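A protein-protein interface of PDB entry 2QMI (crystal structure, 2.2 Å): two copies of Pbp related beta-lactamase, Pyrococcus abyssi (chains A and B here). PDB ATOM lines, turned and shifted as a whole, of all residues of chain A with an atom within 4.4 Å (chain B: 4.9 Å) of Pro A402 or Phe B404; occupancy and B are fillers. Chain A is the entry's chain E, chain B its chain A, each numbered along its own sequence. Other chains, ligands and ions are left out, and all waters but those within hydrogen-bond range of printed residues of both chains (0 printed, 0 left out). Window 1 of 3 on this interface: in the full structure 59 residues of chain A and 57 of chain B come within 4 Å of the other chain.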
ATOM      1  N   VAL A 387     -20.851   0.269  -2.229  1.00  0.00           N
ATOM      2  CA  VAL A 387     -20.229  -0.407  -3.360  1.00  0.00           C
ATOM      3  C   VAL A 387     -18.790  -0.873  -3.155  1.00  0.00           C
ATOM      4  O   VAL A 387     -17.927  -0.114  -2.698  1.00  0.00           O
ATOM      5  CB  VAL A 387     -20.273   0.495  -4.615  1.00  0.00           C
ATOM      6  CG1 VAL A 387     -19.597  -0.208  -5.790  1.00  0.00           C
ATOM      7  CG2 VAL A 387     -21.714   0.845  -4.946  1.00  0.00           C
ATOM      8  N   VAL A 388     -18.551  -2.131  -3.520  1.00  0.00           N
ATOM      9  CA  VAL A 388     -17.235  -2.754  -3.411  1.00  0.00           C
ATOM     10  C   VAL A 388     -16.548  -2.687  -4.770  1.00  0.00           C
ATOM     11  O   VAL A 388     -17.062  -3.227  -5.753  1.00  0.00           O
ATOM     12  CB  VAL A 388     -17.359  -4.243  -3.018  1.00  0.00           C
ATOM     13  CG1 VAL A 388     -15.978  -4.877  -2.920  1.00  0.00           C
ATOM     14  CG2 VAL A 388     -18.113  -4.379  -1.703  1.00  0.00           C
ATOM     15  N   TYR A 389     -15.395  -2.029  -4.836  1.00  0.00           N
ATOM     16  CA  TYR A 389     -14.675  -1.934  -6.104  1.00  0.00           C
ATOM     17  C   TYR A 389     -13.516  -2.933  -6.179  1.00  0.00           C
ATOM     18  O   TYR A 389     -12.742  -3.067  -5.225  1.00  0.00           O
ATOM     19  CB  TYR A 389     -14.142  -0.512  -6.325  1.00  0.00           C
ATOM     20  CG  TYR A 389     -15.224   0.546  -6.440  1.00  0.00           C
ATOM     21  CD1 TYR A 389     -15.809   1.090  -5.298  1.00  0.00           C
ATOM     22  CD2 TYR A 389     -15.672   0.990  -7.690  1.00  0.00           C
ATOM     23  CE1 TYR A 389     -16.813   2.053  -5.388  1.00  0.00           C
ATOM     24  CE2 TYR A 389     -16.683   1.953  -7.793  1.00  0.00           C
ATOM     25  CZ  TYR A 389     -17.248   2.481  -6.633  1.00  0.00           C
ATOM     26  OH  TYR A 389     -18.255   3.428  -6.700  1.00  0.00           O
ATOM     27  N   ILE A 401     -14.037  -2.572 -11.477  1.00  0.00           N
ATOM     28  CA  ILE A 401     -15.318  -3.249 -11.526  1.00  0.00           C
ATOM     29  C   ILE A 401     -16.094  -2.909 -10.256  1.00  0.00           C
ATOM     30  O   ILE A 401     -15.578  -3.056  -9.140  1.00  0.00           O
ATOM     31  CB  ILE A 401     -15.137  -4.788 -11.615  1.00  0.00           C
ATOM     32  CG1 ILE A 401     -14.973  -5.203 -13.079  1.00  0.00           C
ATOM     33  CG2 ILE A 401     -16.318  -5.504 -10.969  1.00  0.00           C
ATOM     34  CD1 ILE A 401     -14.636  -6.673 -13.261  1.00  0.00           C
ATOM     35  N   PRO A 402     -17.331  -2.406 -10.420  1.00  0.00           N
ATOM     36  CA  PRO A 402     -18.186  -2.049  -9.283  1.00  0.00           C
ATOM     37  C   PRO A 402     -18.947  -3.307  -8.873  1.00  0.00           C
ATOM     38  O   PRO A 402     -19.443  -4.044  -9.724  1.00  0.00           O
ATOM     39  CB  PRO A 402     -19.098  -0.971  -9.871  1.00  0.00           C
ATOM     40  CG  PRO A 402     -19.305  -1.465 -11.272  1.00  0.00           C
ATOM     41  CD  PRO A 402     -17.904  -1.910 -11.687  1.00  0.00           C
ATOM     42  N   LEU A 403     -19.018  -3.568  -7.577  1.00  0.00           N
ATOM     43  CA  LEU A 403     -19.714  -4.757  -7.092  1.00  0.00           C
ATOM     44  C   LEU A 403     -20.788  -4.386  -6.071  1.00  0.00           C
ATOM     45  O   LEU A 403     -20.499  -3.806  -5.021  1.00  0.00           O
ATOM     46  CB  LEU A 403     -18.708  -5.736  -6.467  1.00  0.00           C
ATOM     47  CG  LEU A 403     -17.601  -6.287  -7.379  1.00  0.00           C
ATOM     48  CD1 LEU A 403     -16.557  -7.027  -6.535  1.00  0.00           C
ATOM     49  CD2 LEU A 403     -18.206  -7.220  -8.429  1.00  0.00           C
ATOM     50  N   PHE A 404     -22.030  -4.720  -6.403  1.00  0.00           N
ATOM     51  CA  PHE A 404     -23.176  -4.445  -5.555  1.00  0.00           C
ATOM     52  C   PHE A 404     -23.505  -5.675  -4.729  1.00  0.00           C
ATOM     53  O   PHE A 404     -23.950  -6.678  -5.269  1.00  0.00           O
ATOM     54  CB  PHE A 404     -24.400  -4.101  -6.412  1.00  0.00           C
ATOM     55  CG  PHE A 404     -24.339  -2.749  -7.073  1.00  0.00           C
ATOM     56  CD1 PHE A 404     -23.196  -1.960  -6.999  1.00  0.00           C
ATOM     57  CD2 PHE A 404     -25.441  -2.266  -7.774  1.00  0.00           C
ATOM     58  CE1 PHE A 404     -23.156  -0.713  -7.611  1.00  0.00           C
ATOM     59  CE2 PHE A 404     -25.409  -1.022  -8.389  1.00  0.00           C
ATOM     60  CZ  PHE A 404     -24.270  -0.244  -8.308  1.00  0.00           C
ATOM     61  N   TYR A 416     -22.503  -8.638  -7.378  1.00  0.00           N
ATOM     62  CA  TYR A 416     -22.705  -8.771  -8.810  1.00  0.00           C
ATOM     63  C   TYR A 416     -22.398  -7.459  -9.527  1.00  0.00           C
ATOM     64  O   TYR A 416     -22.786  -6.386  -9.072  1.00  0.00           O
ATOM     65  CB  TYR A 416     -24.145  -9.213  -9.099  1.00  0.00           C
ATOM     66  CG  TYR A 416     -25.207  -8.200  -8.718  1.00  0.00           C
ATOM     67  CD1 TYR A 416     -25.679  -7.280  -9.648  1.00  0.00           C
ATOM     68  CD2 TYR A 416     -25.735  -8.160  -7.420  1.00  0.00           C
ATOM     69  CE1 TYR A 416     -26.651  -6.341  -9.310  1.00  0.00           C
ATOM     70  CE2 TYR A 416     -26.712  -7.220  -7.066  1.00  0.00           C
ATOM     71  CZ  TYR A 416     -27.163  -6.315  -8.019  1.00  0.00           C
ATOM     72  OH  TYR A 416     -28.121  -5.380  -7.693  1.00  0.00           O
ATOM     73  N   THR A 417     -21.649  -7.544 -10.619  1.00  0.00           N
ATOM     74  CA  THR A 417     -21.352  -6.358 -11.395  1.00  0.00           C
ATOM     75  C   THR A 417     -22.237  -6.540 -12.610  1.00  0.00           C
ATOM     76  O   THR A 417     -23.090  -7.436 -12.622  1.00  0.00           O
ATOM     77  CB  THR A 417     -19.867  -6.266 -11.821  1.00  0.00           C
ATOM     78  OG1 THR A 417     -19.656  -5.022 -12.507  1.00  0.00           O
ATOM     79  CG2 THR A 417     -19.480  -7.421 -12.740  1.00  0.00           C
ATOM     80  N   LEU A 418     -22.059  -5.714 -13.630  1.00  0.00           N
ATOM     81  CA  LEU A 418     -22.901  -5.857 -14.808  1.00  0.00           C
ATOM     82  C   LEU A 418     -22.026  -6.218 -15.997  1.00  0.00           C
ATOM     83  O   LEU A 418     -21.039  -5.538 -16.289  1.00  0.00           O
ATOM     84  CB  LEU A 418     -23.676  -4.563 -15.053  1.00  0.00           C
ATOM     85  CG  LEU A 418     -25.121  -4.699 -15.535  1.00  0.00           C
ATOM     86  CD1 LEU A 418     -25.935  -5.633 -14.629  1.00  0.00           C
ATOM     87  CD2 LEU A 418     -25.729  -3.311 -15.553  1.00  0.00           C
ATOM     88  N   VAL B 387     -21.455   0.078 -17.494  1.00  0.00           N
ATOM     89  CA  VAL B 387     -21.834   0.912 -16.358  1.00  0.00           C
ATOM     90  C   VAL B 387     -21.853   2.399 -16.655  1.00  0.00           C
ATOM     91  O   VAL B 387     -21.065   2.904 -17.457  1.00  0.00           O
ATOM     92  CB  VAL B 387     -20.899   0.638 -15.146  1.00  0.00           C
ATOM     93  CG1 VAL B 387     -21.148   1.640 -14.034  1.00  0.00           C
ATOM     94  CG2 VAL B 387     -21.141  -0.783 -14.631  1.00  0.00           C
ATOM     95  N   TYR B 389     -21.518   6.128 -15.000  1.00  0.00           N
ATOM     96  CA  TYR B 389     -21.011   6.820 -13.824  1.00  0.00           C
ATOM     97  C   TYR B 389     -21.462   8.267 -13.771  1.00  0.00           C
ATOM     98  O   TYR B 389     -21.349   8.996 -14.756  1.00  0.00           O
ATOM     99  CB  TYR B 389     -19.481   6.785 -13.789  1.00  0.00           C
ATOM    100  CG  TYR B 389     -18.880   5.427 -13.473  1.00  0.00           C
ATOM    101  CD1 TYR B 389     -18.413   4.585 -14.491  1.00  0.00           C
ATOM    102  CD2 TYR B 389     -18.762   4.993 -12.152  1.00  0.00           C
ATOM    103  CE1 TYR B 389     -17.840   3.339 -14.192  1.00  0.00           C
ATOM    104  CE2 TYR B 389     -18.199   3.759 -11.844  1.00  0.00           C
ATOM    105  CZ  TYR B 389     -17.739   2.936 -12.863  1.00  0.00           C
ATOM    106  OH  TYR B 389     -17.192   1.716 -12.533  1.00  0.00           O
ATOM    107  N   PRO B 402     -21.944   4.728  -9.105  1.00  0.00           N
ATOM    108  CA  PRO B 402     -22.032   3.679 -10.127  1.00  0.00           C
ATOM    109  C   PRO B 402     -23.496   3.370 -10.424  1.00  0.00           C
ATOM    110  O   PRO B 402     -24.253   3.040  -9.512  1.00  0.00           O
ATOM    111  CB  PRO B 402     -21.325   2.501  -9.468  1.00  0.00           C
ATOM    112  CG  PRO B 402     -21.764   2.644  -8.039  1.00  0.00           C
ATOM    113  CD  PRO B 402     -21.623   4.144  -7.785  1.00  0.00           C
ATOM    114  N   LEU B 403     -23.896   3.480 -11.689  1.00  0.00           N
ATOM    115  CA  LEU B 403     -25.282   3.206 -12.078  1.00  0.00           C
ATOM    116  C   LEU B 403     -25.431   1.989 -12.996  1.00  0.00           C
ATOM    117  O   LEU B 403     -24.733   1.863 -14.009  1.00  0.00           O
ATOM    118  CB  LEU B 403     -25.889   4.428 -12.772  1.00  0.00           C
ATOM    119  CG  LEU B 403     -25.977   5.743 -11.993  1.00  0.00           C
ATOM    120  CD1 LEU B 403     -26.623   6.790 -12.887  1.00  0.00           C
ATOM    121  CD2 LEU B 403     -26.790   5.562 -10.718  1.00  0.00           C
ATOM    122  N   PHE B 404     -26.354   1.103 -12.641  1.00  0.00           N
ATOM    123  CA  PHE B 404     -26.607  -0.106 -13.416  1.00  0.00           C
ATOM    124  C   PHE B 404     -27.903   0.005 -14.207  1.00  0.00           C
ATOM    125  O   PHE B 404     -28.977   0.130 -13.624  1.00  0.00           O
ATOM    126  CB  PHE B 404     -26.708  -1.315 -12.481  1.00  0.00           C
ATOM    127  CG  PHE B 404     -25.388  -1.788 -11.936  1.00  0.00           C
ATOM    128  CD1 PHE B 404     -24.308  -0.919 -11.820  1.00  0.00           C
ATOM    129  CD2 PHE B 404     -25.243  -3.100 -11.502  1.00  0.00           C
ATOM    130  CE1 PHE B 404     -23.100  -1.350 -11.276  1.00  0.00           C
ATOM    131  CE2 PHE B 404     -24.043  -3.544 -10.957  1.00  0.00           C
ATOM    132  CZ  PHE B 404     -22.968  -2.667 -10.843  1.00  0.00           C
ATOM    133  N   PRO B 405     -27.824  -0.040 -15.547  1.00  0.00           N
ATOM    134  CA  PRO B 405     -29.041   0.056 -16.355  1.00  0.00           C
ATOM    135  C   PRO B 405     -29.951  -1.138 -16.105  1.00  0.00           C
ATOM    136  O   PRO B 405     -29.521  -2.283 -16.223  1.00  0.00           O
ATOM    137  CB  PRO B 405     -28.502   0.086 -17.783  1.00  0.00           C
ATOM    138  CG  PRO B 405     -27.185   0.760 -17.627  1.00  0.00           C
ATOM    139  CD  PRO B 405     -26.629   0.073 -16.402  1.00  0.00           C
ATOM    140  N   GLU B 406     -31.205  -0.864 -15.750  1.00  0.00           N
ATOM    141  CA  GLU B 406     -32.185  -1.908 -15.477  1.00  0.00           C
ATOM    142  C   GLU B 406     -33.227  -1.871 -16.576  1.00  0.00           C
ATOM    143  O   GLU B 406     -33.989  -2.820 -16.747  1.00  0.00           O
ATOM    144  CB  GLU B 406     -32.867  -1.665 -14.128  1.00  0.00           C
ATOM    145  CG  GLU B 406     -33.988  -2.647 -13.784  1.00  0.00           C
ATOM    146  CD  GLU B 406     -34.894  -2.130 -12.662  1.00  0.00           C
ATOM    147  OE1 GLU B 406     -34.424  -2.020 -11.503  1.00  0.00           O
ATOM    148  OE2 GLU B 406     -36.082  -1.823 -12.936  1.00  0.00           O
ATOM    149  N   LYS B 414     -33.411   3.638 -17.488  1.00  0.00           N
ATOM    150  CA  LYS B 414     -33.614   3.650 -16.046  1.00  0.00           C
ATOM    151  C   LYS B 414     -32.453   2.896 -15.406  1.00  0.00           C
ATOM    152  O   LYS B 414     -32.180   1.752 -15.764  1.00  0.00           O
ATOM    153  CB  LYS B 414     -34.943   2.983 -15.686  1.00  0.00           C
ATOM    154  CG  LYS B 414     -35.269   3.015 -14.206  1.00  0.00           C
ATOM    155  CD  LYS B 414     -36.695   2.552 -13.930  1.00  0.00           C
ATOM    156  CE  LYS B 414     -37.064   2.740 -12.465  1.00  0.00           C
ATOM    157  NZ  LYS B 414     -38.476   2.351 -12.178  1.00  0.00           N
ATOM    158  N   CYS B 415     -31.755   3.545 -14.480  1.00  0.00           N
ATOM    159  CA  CYS B 415     -30.622   2.925 -13.806  1.00  0.00           C
ATOM    160  C   CYS B 415     -30.858   2.917 -12.311  1.00  0.00           C
ATOM    161  O   CYS B 415     -31.801   3.539 -11.818  1.00  0.00           O
ATOM    162  CB  CYS B 415     -29.330   3.698 -14.076  1.00  0.00           C
ATOM    163  SG  CYS B 415     -28.943   3.920 -15.799  1.00  0.00           S
ATOM    164  N   TYR B 416     -29.990   2.217 -11.593  1.00  0.00           N
ATOM    165  CA  TYR B 416     -30.097   2.145 -10.144  1.00  0.00           C
ATOM    166  C   TYR B 416     -28.713   1.951  -9.574  1.00  0.00           C
ATOM    167  O   TYR B 416     -27.821   1.420 -10.240  1.00  0.00           O
ATOM    168  CB  TYR B 416     -30.995   0.977  -9.726  1.00  0.00           C
ATOM    169  CG  TYR B 416     -30.389  -0.391  -9.953  1.00  0.00           C
ATOM    170  CD1 TYR B 416     -29.522  -0.957  -9.016  1.00  0.00           C
ATOM    171  CD2 TYR B 416     -30.680  -1.122 -11.107  1.00  0.00           C
ATOM    172  CE1 TYR B 416     -28.961  -2.217  -9.217  1.00  0.00           C
ATOM    173  CE2 TYR B 416     -30.120  -2.392 -11.321  1.00  0.00           C
ATOM    174  CZ  TYR B 416     -29.262  -2.928 -10.366  1.00  0.00           C
ATOM    175  OH  TYR B 416     -28.709  -4.178 -10.559  1.00  0.00           O
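The side-chain hydroxyl (OH) of Tyr B416 is in hydrogen-bond range of the side-chain hydroxyl (OH) of Tyr A416 (3.2 Å).
Among the printed residues, merely in contact across the chains: Val A387 with Pro B402, Tyr A389 with Pro B402, Pro A402 with Val B387, Pro A402 with Tyr B389, Pro A402 with Phe B404, Phe A404 with Pro B402, Phe A404 with Phe B404, Phe A404 with Tyr B416, Tyr A416 with Phe B404, Thr A417 with Phe B404, Leu A418 with Phe B404 and Leu A418 with Pro B405.
Of the printed residues of chain B, Phe A404 touches Pro B402 (3.5 Å), Phe B404 (3.4 Å) and Tyr B416 (3.8 Å).
Of the printed residues of chain B, Tyr A416 touches Phe B404 and Tyr B416.
Of the printed residues of chain A, Val B387 touches Pro A402.
Of the printed residues of chain A, Pro B402 touches Val A387, Tyr A389 and Phe A404.
The nearest residue of chain B that does not touch Pro A402 is Pro B402 (4.1 Å).
The nearest printed residue of chain B that does not touch Tyr A389 is Tyr B389 (4.7 Å).
Tyr A389 touches Pro B402, and with the chains exchanged Pro A402 touches Tyr B389.
Phe A404 touches its own counterpart, Phe B404.
Phe A404 touches Tyr B416, and with the chains exchanged Tyr A416 touches Phe B404.
Tyr A416 touches its own counterpart, Tyr B416.
Hydrophobic or aromatic side chains of chain B within 4 Å of the printed part of chain A: Val B387, Tyr B389, Pro B402, Phe B404, Pro B405 and Tyr B416.
Along chain B the printed residues that touch a printed residue of chain A span positions 387 to 416.
Hydrophobic or aromatic side chains of chain A that line the printed part of chain B: Val A387, Tyr A389, Pro A402, Phe A404, Tyr A416 and Leu A418.
Along chain A the printed residues that touch a printed residue of chain B span positions 387 to 418.
Among the printed residues, 13 pairs touch across the chains.
Among the printed residues, no Asp or Glu carboxylate lies within 4 Å of a Lys or Arg side-chain nitrogen of the other chain.
The backbone carbonyl oxygen of Pro A402 is in hydrogen-bond range of the side-chain hydroxyl of Thr A417, at 3.0 Å.
O of Tyr B416 lies within hydrogen-bond range of N of Phe B404 (2.8 Å).
O of Phe A404 sits close to N of Tyr A416, 3.2 Å away.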
